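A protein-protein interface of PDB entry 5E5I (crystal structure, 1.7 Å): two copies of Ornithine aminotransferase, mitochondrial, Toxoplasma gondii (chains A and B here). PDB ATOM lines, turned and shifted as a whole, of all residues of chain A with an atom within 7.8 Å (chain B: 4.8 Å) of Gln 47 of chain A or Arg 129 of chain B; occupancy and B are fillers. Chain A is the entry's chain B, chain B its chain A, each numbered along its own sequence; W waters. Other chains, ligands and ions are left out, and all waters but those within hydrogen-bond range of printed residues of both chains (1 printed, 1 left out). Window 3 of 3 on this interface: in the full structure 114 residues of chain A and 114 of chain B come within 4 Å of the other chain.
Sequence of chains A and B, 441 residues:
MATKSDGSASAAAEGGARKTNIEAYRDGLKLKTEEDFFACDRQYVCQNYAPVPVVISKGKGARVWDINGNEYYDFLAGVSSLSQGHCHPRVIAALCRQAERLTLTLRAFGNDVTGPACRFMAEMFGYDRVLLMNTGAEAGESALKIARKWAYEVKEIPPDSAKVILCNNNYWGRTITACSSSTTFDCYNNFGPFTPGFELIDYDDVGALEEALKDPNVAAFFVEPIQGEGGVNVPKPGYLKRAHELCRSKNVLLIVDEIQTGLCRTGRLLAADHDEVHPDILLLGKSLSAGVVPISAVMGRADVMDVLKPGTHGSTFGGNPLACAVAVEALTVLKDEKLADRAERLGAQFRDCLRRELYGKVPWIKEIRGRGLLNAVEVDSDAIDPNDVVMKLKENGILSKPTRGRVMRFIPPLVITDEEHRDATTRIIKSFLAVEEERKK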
ATOM      1  N   ALA A  39       9.127  -6.814  -0.694  1.00  0.00           N
ATOM      2  CA  ALA A  39       9.895  -7.296   0.443  1.00  0.00           C
ATOM      3  C   ALA A  39       9.608  -8.764   0.753  1.00  0.00           C
ATOM      4  O   ALA A  39      10.536  -9.522   1.068  1.00  0.00           O
ATOM      5  CB  ALA A  39       9.647  -6.450   1.687  1.00  0.00           C
ATOM      6  N   CYS A  40       8.330  -9.128   0.717  1.00  0.00           N
ATOM      7  CA  CYS A  40       7.900 -10.509   1.005  1.00  0.00           C
ATOM      8  C   CYS A  40       8.574 -11.432   0.009  1.00  0.00           C
ATOM      9  O   CYS A  40       9.263 -12.419   0.344  1.00  0.00           O
ATOM     10  CB  CYS A  40       6.381 -10.594   0.944  1.00  0.00           C
ATOM     11  SG  CYS A  40       5.661 -12.222   1.209  1.00  0.00           S
ATOM     12  N   ASP A  41       8.459 -11.014  -1.236  1.00  0.00           N
ATOM     13  CA  ASP A  41       9.055 -11.747  -2.285  1.00  0.00           C
ATOM     14  C   ASP A  41      10.585 -11.862  -2.075  1.00  0.00           C
ATOM     15  O   ASP A  41      11.105 -12.961  -2.153  1.00  0.00           O
ATOM     16  CB  ASP A  41       8.586 -11.198  -3.640  1.00  0.00           C
ATOM     17  CG  ASP A  41       9.098 -12.001  -4.758  1.00  0.00           C
ATOM     18  OD1 ASP A  41      10.338 -11.961  -4.907  1.00  0.00           O
ATOM     19  OD2 ASP A  41       8.288 -12.690  -5.442  1.00  0.00           O
ATOM     20  N   ARG A  42      11.290 -10.787  -1.699  1.00  0.00           N
ATOM     21  CA  ARG A  42      12.751 -10.887  -1.462  1.00  0.00           C
ATOM     22  C   ARG A  42      13.143 -11.803  -0.328  1.00  0.00           C
ATOM     23  O   ARG A  42      14.205 -12.415  -0.359  1.00  0.00           O
ATOM     24  CB  ARG A  42      13.436  -9.531  -1.163  1.00  0.00           C
ATOM     25  CG  ARG A  42      13.847  -8.688  -2.368  1.00  0.00           C
ATOM     26  CD  ARG A  42      14.658  -7.440  -1.973  1.00  0.00           C
ATOM     27  NE  ARG A  42      14.023  -6.614  -0.927  1.00  0.00           N
ATOM     28  CZ  ARG A  42      13.085  -5.665  -1.099  1.00  0.00           C
ATOM     29  NH1 ARG A  42      12.582  -5.357  -2.294  1.00  0.00           N
ATOM     30  NH2 ARG A  42      12.619  -5.018  -0.038  1.00  0.00           N
ATOM     31  N   GLN A  43      12.329 -11.878   0.713  1.00  0.00           N
ATOM     32  CA  GLN A  43      12.693 -12.693   1.846  1.00  0.00           C
ATOM     33  C   GLN A  43      12.391 -14.208   1.732  1.00  0.00           C
ATOM     34  O   GLN A  43      13.130 -15.010   2.281  1.00  0.00           O
ATOM     35  CB  GLN A  43      11.960 -12.155   3.056  1.00  0.00           C
ATOM     36  CG  GLN A  43      12.153 -12.958   4.321  1.00  0.00           C
ATOM     37  CD  GLN A  43      11.642 -12.182   5.509  1.00  0.00           C
ATOM     38  OE1 GLN A  43      10.694 -11.374   5.390  1.00  0.00           O
ATOM     39  NE2 GLN A  43      12.295 -12.365   6.654  1.00  0.00           N
ATOM     40  N   TYR A  44      11.307 -14.584   1.067  1.00  0.00           N
ATOM     41  CA  TYR A  44      10.895 -15.984   1.045  1.00  0.00           C
ATOM     42  C   TYR A  44      10.954 -16.694  -0.279  1.00  0.00           C
ATOM     43  O   TYR A  44      10.896 -17.908  -0.313  1.00  0.00           O
ATOM     44  CB  TYR A  44       9.453 -16.082   1.579  1.00  0.00           C
ATOM     45  CG  TYR A  44       9.297 -15.539   2.949  1.00  0.00           C
ATOM     46  CD1 TYR A  44       9.763 -16.260   4.049  1.00  0.00           C
ATOM     47  CD2 TYR A  44       8.724 -14.276   3.171  1.00  0.00           C
ATOM     48  CE1 TYR A  44       9.654 -15.753   5.344  1.00  0.00           C
ATOM     49  CE2 TYR A  44       8.631 -13.756   4.455  1.00  0.00           C
ATOM     50  CZ  TYR A  44       9.069 -14.512   5.536  1.00  0.00           C
ATOM     51  OH  TYR A  44       8.978 -14.006   6.829  1.00  0.00           O
ATOM     52  N   VAL A  45      11.100 -15.967  -1.375  1.00  0.00           N
ATOM     53  CA  VAL A  45      11.073 -16.575  -2.689  1.00  0.00           C
ATOM     54  C   VAL A  45      12.502 -16.721  -3.173  1.00  0.00           C
ATOM     55  O   VAL A  45      13.284 -15.825  -3.047  1.00  0.00           O
ATOM     56  CB  VAL A  45      10.261 -15.742  -3.676  1.00  0.00           C
ATOM     57  CG1 VAL A  45      10.191 -16.426  -5.038  1.00  0.00           C
ATOM     58  CG2 VAL A  45       8.827 -15.548  -3.159  1.00  0.00           C
ATOM     59  N   CYS A  46      12.821 -17.880  -3.688  1.00  0.00           N
ATOM     60  CA  CYS A  46      14.164 -18.103  -4.283  1.00  0.00           C
ATOM     61  C   CYS A  46      14.405 -16.904  -5.222  1.00  0.00           C
ATOM     62  O   CYS A  46      13.572 -16.610  -6.068  1.00  0.00           O
ATOM     63  CB  CYS A  46      14.122 -19.414  -5.049  1.00  0.00           C
ATOM     64  SG  CYS A  46      15.709 -19.858  -5.734  1.00  0.00           S
ATOM     65  N   GLN A  47      15.566 -16.267  -5.098  1.00  0.00           N
ATOM     66  CA  GLN A  47      15.889 -15.011  -5.818  1.00  0.00           C
ATOM     67  C   GLN A  47      16.470 -15.206  -7.251  1.00  0.00           C
ATOM     68  O   GLN A  47      17.370 -14.509  -7.674  1.00  0.00           O
ATOM     69  CB  GLN A  47      16.814 -14.165  -4.919  1.00  0.00           C
ATOM     70  CG  GLN A  47      16.226 -13.850  -3.520  1.00  0.00           C
ATOM     71  CD  GLN A  47      17.186 -13.190  -2.463  1.00  0.00           C
ATOM     72  OE1 GLN A  47      16.714 -12.503  -1.520  1.00  0.00           O
ATOM     73  NE2 GLN A  47      18.491 -13.395  -2.599  1.00  0.00           N
ATOM     74  N   ASN A  48      15.862 -16.112  -8.021  1.00  0.00           N
ATOM     75  CA  ASN A  48      16.339 -16.394  -9.371  1.00  0.00           C
ATOM     76  C   ASN A  48      15.719 -15.535 -10.457  1.00  0.00           C
ATOM     77  O   ASN A  48      15.974 -15.760 -11.634  1.00  0.00           O
ATOM     78  CB  ASN A  48      16.242 -17.877  -9.696  1.00  0.00           C
ATOM     79  CG  ASN A  48      14.856 -18.390  -9.654  1.00  0.00           C
ATOM     80  OD1 ASN A  48      14.200 -18.411  -8.602  1.00  0.00           O
ATOM     81  ND2 ASN A  48      14.380 -18.858 -10.799  1.00  0.00           N
ATOM     82  N   TYR A  49      14.880 -14.560 -10.079  1.00  0.00           N
ATOM     83  CA  TYR A  49      14.369 -13.598 -11.048  1.00  0.00           C
ATOM     84  C   TYR A  49      14.766 -12.201 -10.673  1.00  0.00           C
ATOM     85  O   TYR A  49      14.849 -11.894  -9.498  1.00  0.00           O
ATOM     86  CB  TYR A  49      12.856 -13.695 -11.196  1.00  0.00           C
ATOM     87  CG  TYR A  49      12.437 -14.808 -12.107  1.00  0.00           C
ATOM     88  CD1 TYR A  49      12.386 -16.144 -11.664  1.00  0.00           C
ATOM     89  CD2 TYR A  49      12.077 -14.536 -13.424  1.00  0.00           C
ATOM     90  CE1 TYR A  49      12.012 -17.166 -12.537  1.00  0.00           C
ATOM     91  CE2 TYR A  49      11.660 -15.546 -14.279  1.00  0.00           C
ATOM     92  CZ  TYR A  49      11.630 -16.848 -13.826  1.00  0.00           C
ATOM     93  OH  TYR A  49      11.251 -17.803 -14.718  1.00  0.00           O
ATOM     94  N   ALA A  50      14.956 -11.343 -11.666  1.00  0.00           N
ATOM     95  CA  ALA A  50      15.299  -9.951 -11.412  1.00  0.00           C
ATOM     96  C   ALA A  50      14.153  -9.194 -10.736  1.00  0.00           C
ATOM     97  O   ALA A  50      12.996  -9.677 -10.700  1.00  0.00           O
ATOM     98  CB  ALA A  50      15.699  -9.247 -12.715  1.00  0.00           C
ATOM     99  N   PRO A  51      14.479  -8.003 -10.173  1.00  0.00           N
ATOM    100  CA  PRO A  51      13.418  -7.228  -9.562  1.00  0.00           C
ATOM    101  C   PRO A  51      12.297  -6.960 -10.573  1.00  0.00           C
ATOM    102  O   PRO A  51      12.511  -6.822 -11.779  1.00  0.00           O
ATOM    103  CB  PRO A  51      14.130  -5.926  -9.093  1.00  0.00           C
ATOM    104  CG  PRO A  51      15.571  -6.318  -8.893  1.00  0.00           C
ATOM    105  CD  PRO A  51      15.811  -7.369  -9.971  1.00  0.00           C
ATOM    106  N   TYR B 127      12.075 -23.191   6.299  1.00  0.00           N
ATOM    107  CA  TYR B 127      13.190 -22.915   5.344  1.00  0.00           C
ATOM    108  C   TYR B 127      13.194 -21.437   5.063  1.00  0.00           C
ATOM    109  O   TYR B 127      12.169 -20.789   5.174  1.00  0.00           O
ATOM    110  CB  TYR B 127      13.027 -23.716   4.056  1.00  0.00           C
ATOM    111  CG  TYR B 127      13.353 -25.140   4.263  1.00  0.00           C
ATOM    112  CD1 TYR B 127      14.667 -25.563   4.189  1.00  0.00           C
ATOM    113  CD2 TYR B 127      12.393 -26.077   4.614  1.00  0.00           C
ATOM    114  CE1 TYR B 127      14.998 -26.890   4.388  1.00  0.00           C
ATOM    115  CE2 TYR B 127      12.730 -27.397   4.845  1.00  0.00           C
ATOM    116  CZ  TYR B 127      14.025 -27.797   4.735  1.00  0.00           C
ATOM    117  OH  TYR B 127      14.402 -29.101   4.961  1.00  0.00           O
ATOM    118  N   ASP B 128      14.329 -20.927   4.644  1.00  0.00           N
ATOM    119  CA  ASP B 128      14.466 -19.528   4.348  1.00  0.00           C
ATOM    120  C   ASP B 128      13.890 -19.141   2.944  1.00  0.00           C
ATOM    121  O   ASP B 128      13.390 -18.049   2.757  1.00  0.00           O
ATOM    122  CB  ASP B 128      15.980 -19.189   4.267  1.00  0.00           C
ATOM    123  CG  ASP B 128      16.715 -19.268   5.615  1.00  0.00           C
ATOM    124  OD1 ASP B 128      16.101 -19.021   6.650  1.00  0.00           O
ATOM    125  OD2 ASP B 128      17.966 -19.454   5.656  1.00  0.00           O
ATOM    126  N   ARG B 129      14.125 -20.005   1.954  1.00  0.00           N
ATOM    127  CA  ARG B 129      13.749 -19.712   0.566  1.00  0.00           C
ATOM    128  C   ARG B 129      13.054 -20.880  -0.066  1.00  0.00           C
ATOM    129  O   ARG B 129      13.450 -22.043   0.121  1.00  0.00           O
ATOM    130  CB  ARG B 129      14.971 -19.471  -0.352  1.00  0.00           C
ATOM    131  CG  ARG B 129      15.984 -18.456   0.112  1.00  0.00           C
ATOM    132  CD  ARG B 129      15.513 -17.006  -0.113  1.00  0.00           C
ATOM    133  NE  ARG B 129      16.672 -16.171   0.154  1.00  0.00           N
ATOM    134  CZ  ARG B 129      16.905 -15.472   1.260  1.00  0.00           C
ATOM    135  NH1 ARG B 129      15.968 -15.274   2.183  1.00  0.00           N
ATOM    136  NH2 ARG B 129      18.064 -14.806   1.354  1.00  0.00           N
ATOM    137  N   VAL B 130      12.046 -20.545  -0.870  1.00  0.00           N
ATOM    138  CA  VAL B 130      11.252 -21.525  -1.578  1.00  0.00           C
ATOM    139  C   VAL B 130      11.294 -21.283  -3.083  1.00  0.00           C
ATOM    140  O   VAL B 130      10.961 -20.193  -3.555  1.00  0.00           O
ATOM    141  CB  VAL B 130       9.750 -21.459  -1.123  1.00  0.00           C
ATOM    142  CG1 VAL B 130       8.840 -22.398  -1.956  1.00  0.00           C
ATOM    143  CG2 VAL B 130       9.623 -21.809   0.354  1.00  0.00           C
ATOM    144  N   LEU B 131      11.664 -22.303  -3.819  1.00  0.00           N
ATOM    145  CA  LEU B 131      11.624 -22.269  -5.252  1.00  0.00           C
ATOM    146  C   LEU B 131      10.457 -23.110  -5.739  1.00  0.00           C
ATOM    147  O   LEU B 131      10.444 -24.309  -5.521  1.00  0.00           O
ATOM    148  CB  LEU B 131      12.906 -22.871  -5.858  1.00  0.00           C
ATOM    149  CG  LEU B 131      12.910 -23.110  -7.366  1.00  0.00           C
ATOM    150  CD1 LEU B 131      12.871 -21.818  -8.095  1.00  0.00           C
ATOM    151  CD2 LEU B 131      14.225 -23.848  -7.751  1.00  0.00           C
ATOM    152  N   VAL B 298      11.134 -26.712  -4.006  1.00  0.00           N
ATOM    153  CA  VAL B 298      12.549 -26.999  -3.594  1.00  0.00           C
ATOM    154  C   VAL B 298      12.790 -25.959  -2.536  1.00  0.00           C
ATOM    155  O   VAL B 298      12.621 -24.745  -2.800  1.00  0.00           O
ATOM    156  CB  VAL B 298      13.500 -26.812  -4.732  1.00  0.00           C
ATOM    157  CG1 VAL B 298      14.911 -27.060  -4.278  1.00  0.00           C
ATOM    158  CG2 VAL B 298      13.152 -27.807  -5.846  1.00  0.00           C
ATOM    159  N   MET B 299      13.132 -26.381  -1.316  1.00  0.00           N
ATOM    160  CA  MET B 299      13.332 -25.427  -0.209  1.00  0.00           C
ATOM    161  C   MET B 299      14.684 -25.665   0.442  1.00  0.00           C
ATOM    162  O   MET B 299      15.117 -26.814   0.571  1.00  0.00           O
ATOM    163  CB  MET B 299      12.250 -25.569   0.879  1.00  0.00           C
ATOM    164  CG  MET B 299      10.871 -25.511   0.324  1.00  0.00           C
ATOM    165  SD  MET B 299       9.608 -25.584   1.596  1.00  0.00           S
ATOM    166  CE  MET B 299       8.242 -25.956   0.494  1.00  0.00           C
ATOM    167  N   GLY B 300      15.270 -24.573   0.906  1.00  0.00           N
ATOM    168  CA  GLY B 300      16.613 -24.625   1.497  1.00  0.00           C
ATOM    169  C   GLY B 300      16.991 -23.368   2.231  1.00  0.00           C
ATOM    170  O   GLY B 300      16.304 -22.352   2.171  1.00  0.00           O
ATOM    171  N   ALA B 302      19.152 -19.999   3.054  1.00  0.00           N
ATOM    172  CA  ALA B 302      19.561 -18.900   2.206  1.00  0.00           C
ATOM    173  C   ALA B 302      20.914 -19.047   1.533  1.00  0.00           C
ATOM    174  O   ALA B 302      21.038 -18.805   0.325  1.00  0.00           O
ATOM    175  CB  ALA B 302      19.531 -17.610   2.993  1.00  0.00           C
ATOM    176  N   MET B 305      20.323 -21.832  -1.327  1.00  0.00           N
ATOM    177  CA  MET B 305      19.409 -21.419  -2.389  1.00  0.00           C
ATOM    178  C   MET B 305      19.789 -20.124  -3.142  1.00  0.00           C
ATOM    179  O   MET B 305      19.388 -19.947  -4.296  1.00  0.00           O
ATOM    180  CB  MET B 305      18.000 -21.253  -1.788  1.00  0.00           C
ATOM    181  CG  MET B 305      17.488 -22.531  -1.158  1.00  0.00           C
ATOM    182  SD  MET B 305      17.106 -23.868  -2.285  1.00  0.00           S
ATOM    183  CE  MET B 305      15.703 -23.153  -3.125  1.00  0.00           C
ATOM    184  N   ASP B 306      20.511 -19.214  -2.509  1.00  0.00           N
ATOM    185  CA  ASP B 306      20.830 -17.901  -3.128  1.00  0.00           C
ATOM    186  C   ASP B 306      21.852 -18.014  -4.239  1.00  0.00           C
ATOM    187  O   ASP B 306      22.110 -17.011  -4.906  1.00  0.00           O
ATOM    188  CB  ASP B 306      21.239 -16.834  -2.089  1.00  0.00           C
ATOM    189  CG  ASP B 306      20.032 -16.338  -1.173  1.00  0.00           C
ATOM    190  OD1 ASP B 306      18.849 -16.675  -1.443  1.00  0.00           O
ATOM    191  OD2 ASP B 306      20.304 -15.558  -0.227  1.00  0.00           O
ATOM    192  N   LEU B 308      21.247 -19.456  -6.868  1.00  0.00           N
ATOM    193  CA  LEU B 308      20.401 -19.271  -8.073  1.00  0.00           C
ATOM    194  C   LEU B 308      20.077 -17.797  -8.279  1.00  0.00           C
ATOM    195  O   LEU B 308      18.980 -17.311  -7.923  1.00  0.00           O
ATOM    196  CB  LEU B 308      19.099 -20.065  -7.996  1.00  0.00           C
ATOM    197  CG  LEU B 308      19.147 -21.599  -8.064  1.00  0.00           C
ATOM    198  CD1 LEU B 308      17.746 -22.110  -8.360  1.00  0.00           C
ATOM    199  CD2 LEU B 308      20.088 -22.125  -9.135  1.00  0.00           C
ATOM    200  N   LYS B 309      21.032 -17.087  -8.853  1.00  0.00           N
ATOM    201  CA  LYS B 309      20.919 -15.663  -9.136  1.00  0.00           C
ATOM    202  C   LYS B 309      20.005 -15.377 -10.333  1.00  0.00           C
ATOM    203  O   LYS B 309      19.752 -16.277 -11.132  1.00  0.00           O
ATOM    204  CB  LYS B 309      22.304 -15.081  -9.442  1.00  0.00           C
ATOM    205  CG  LYS B 309      23.296 -15.091  -8.281  1.00  0.00           C
ATOM    206  CD  LYS B 309      22.866 -14.200  -7.117  1.00  0.00           C
ATOM    207  CE  LYS B 309      23.987 -14.098  -6.060  1.00  0.00           C
ATOM    208  NZ  LYS B 309      24.520 -15.422  -5.625  1.00  0.00           N
ATOM    209  N   PRO B 310      19.552 -14.112 -10.475  1.00  0.00           N
ATOM    210  CA  PRO B 310      18.678 -13.778 -11.614  1.00  0.00           C
ATOM    211  C   PRO B 310      19.188 -14.241 -12.956  1.00  0.00           C
ATOM    212  O   PRO B 310      20.366 -14.055 -13.291  1.00  0.00           O
ATOM    213  CB  PRO B 310      18.601 -12.258 -11.572  1.00  0.00           C
ATOM    214  CG  PRO B 310      18.824 -11.913 -10.141  1.00  0.00           C
ATOM    215  CD  PRO B 310      19.740 -12.946  -9.582  1.00  0.00           C
HETATM  216  O   HOH W   1      17.390 -17.983  -3.397  1.00  0.00           O
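Asp 41 of chain A touches none of the printed residues of chain B.
Printed residues of chain B within 4 Å of Gln 43 of chain A: Asp 128 (3.1 Å) and Arg 129 (2.9 Å).
Gln 47 of chain A touches five residues of chain B.
Of the printed residues of chain B, Ala 50 of chain A touches Pro 310.
Of the printed residues of chain A, Asp 128 of chain B touches Gln 43 and Tyr 44.
Of chain A, only Gln 43, Tyr 44, Val 45 and Gln 47 come within 4 Å of Arg 129 of chain B.
Of the printed residues of chain A, Val 130 of chain B touches Tyr 44, Val 45 and Cys 46.
The nearest printed residue of chain B that does not touch Gln 47 of chain A is Met 305 of chain B (5.4 Å).
No position is printed for both chains.
Of the 21 pairs that touch across the chains among the printed residues, none has its exchanged pair printed and touching as well.
Water W1 lies within hydrogen-bond range of OD1 of Asp 306 of chain B (2.8 Å), O of Met 305 of chain B (2.9 Å), N of Gln 47 of chain A (3.0 Å) and SG of Cys 46 of chain A (3.4 Å).
The guanidinium group (NH1) of Arg 129 of chain B lies within hydrogen-bond range of the backbone carbonyl oxygen (O) of Gln 43 of chain A, at 2.9 Å.
The backbone NH of Val 130 of chain B sits at hydrogen-bond distance from the backbone carbonyl oxygen of Tyr 44 of chain A, at 2.9 Å.
N of Cys 46 of chain A sits at hydrogen-bond distance from O of Val 130 of chain B (3.0 Å).
OD1 of Asp 306 of chain B lies within hydrogen-bond range of NE2 of Gln 47 of chain A, 3.5 Å away.
The backbone NH of Asn 48 of chain A sits close to the backbone carbonyl oxygen of Leu 308 of chain B, 3.3 Å away.
O of Asp 128 of chain B sits close to O of Gln 43 of chain A, at 3.1 Å.
The backbone carbonyl oxygen of Gln 47 of chain A lies close to the backbone carbonyl oxygen of Leu 308 of chain B, 3.2 Å away.
Printed residues of chain B that touch a printed residue of chain A: Asp 128, Arg 129, Val 130, Leu 131, Met 305, Asp 306, Leu 308, Lys 309 and Pro 310.
Hydrophobic or aromatic side chains of chain B that line the printed part of chain A: Val 130, Leu 131, Leu 308 and Pro 310.
Among the printed residues, 21 pairs touch across the chains.
Among the printed residues, no Asp or Glu carboxylate lies within 4 Å of a Lys or Arg side-chain nitrogen of the other chain.
O of Gly 300 of chain B is in hydrogen-bond range of N of Asp 128 of chain B, at 3.5 Å.
OD2 of Asp 128 of chain B is in hydrogen-bond range of N of Ala 302 of chain B (2.9 Å).
OD1 of Asp 306 of chain B is in salt-bridge range of NE of Arg 129 of chain B, 2.7 Å away.
The side-chain sulfur (SD) of Met 305 of chain B sits close to the backbone NH (N) of Gly 300 of chain B, 3.7 Å away.
The backbone carbonyl oxygen (O) of Arg 42 of chain A sits close to the side-chain amide oxygen (OE1) of Gln 47 of chain A (2.8 Å).
The backbone carbonyl oxygen of Cys 46 of chain A lies close to the side-chain amide oxygen of Asn 48 of chain A (3.2 Å).
Among the printed residues, pairs that only touch across the chains: Tyr 44 of chain A with Asp 128 of chain B (3.7 Å), Tyr 44 of chain A with Arg 129 of chain B (3.5 Å), Val 45 of chain A with Arg 129 of chain B (3.9 Å), Val 45 of chain A with Val 130 of chain B (3.7 Å), Cys 46 of chain A with Leu 131 of chain B (3.8 Å), Cys 46 of chain A with Met 305 of chain B (3.95 Å), Gln 47 of chain A with Arg 129 of chain B (3.9 Å), Gln 47 of chain A with Lys 309 of chain B (3.8 Å), Gln 47 of chain A with Pro 310 of chain B (3.4 Å), Asn 48 of chain A with Leu 131 of chain B (3.7 Å), Asn 48 of chain A with Lys 309 of chain B (3.8 Å), Asn 48 of chain A with Pro 310 of chain B (3.4 Å), Tyr 49 of chain A with Pro 310 of chain B (3.9 Å) and Ala 50 of chain A with Pro 310 of chain B (3.8 Å).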
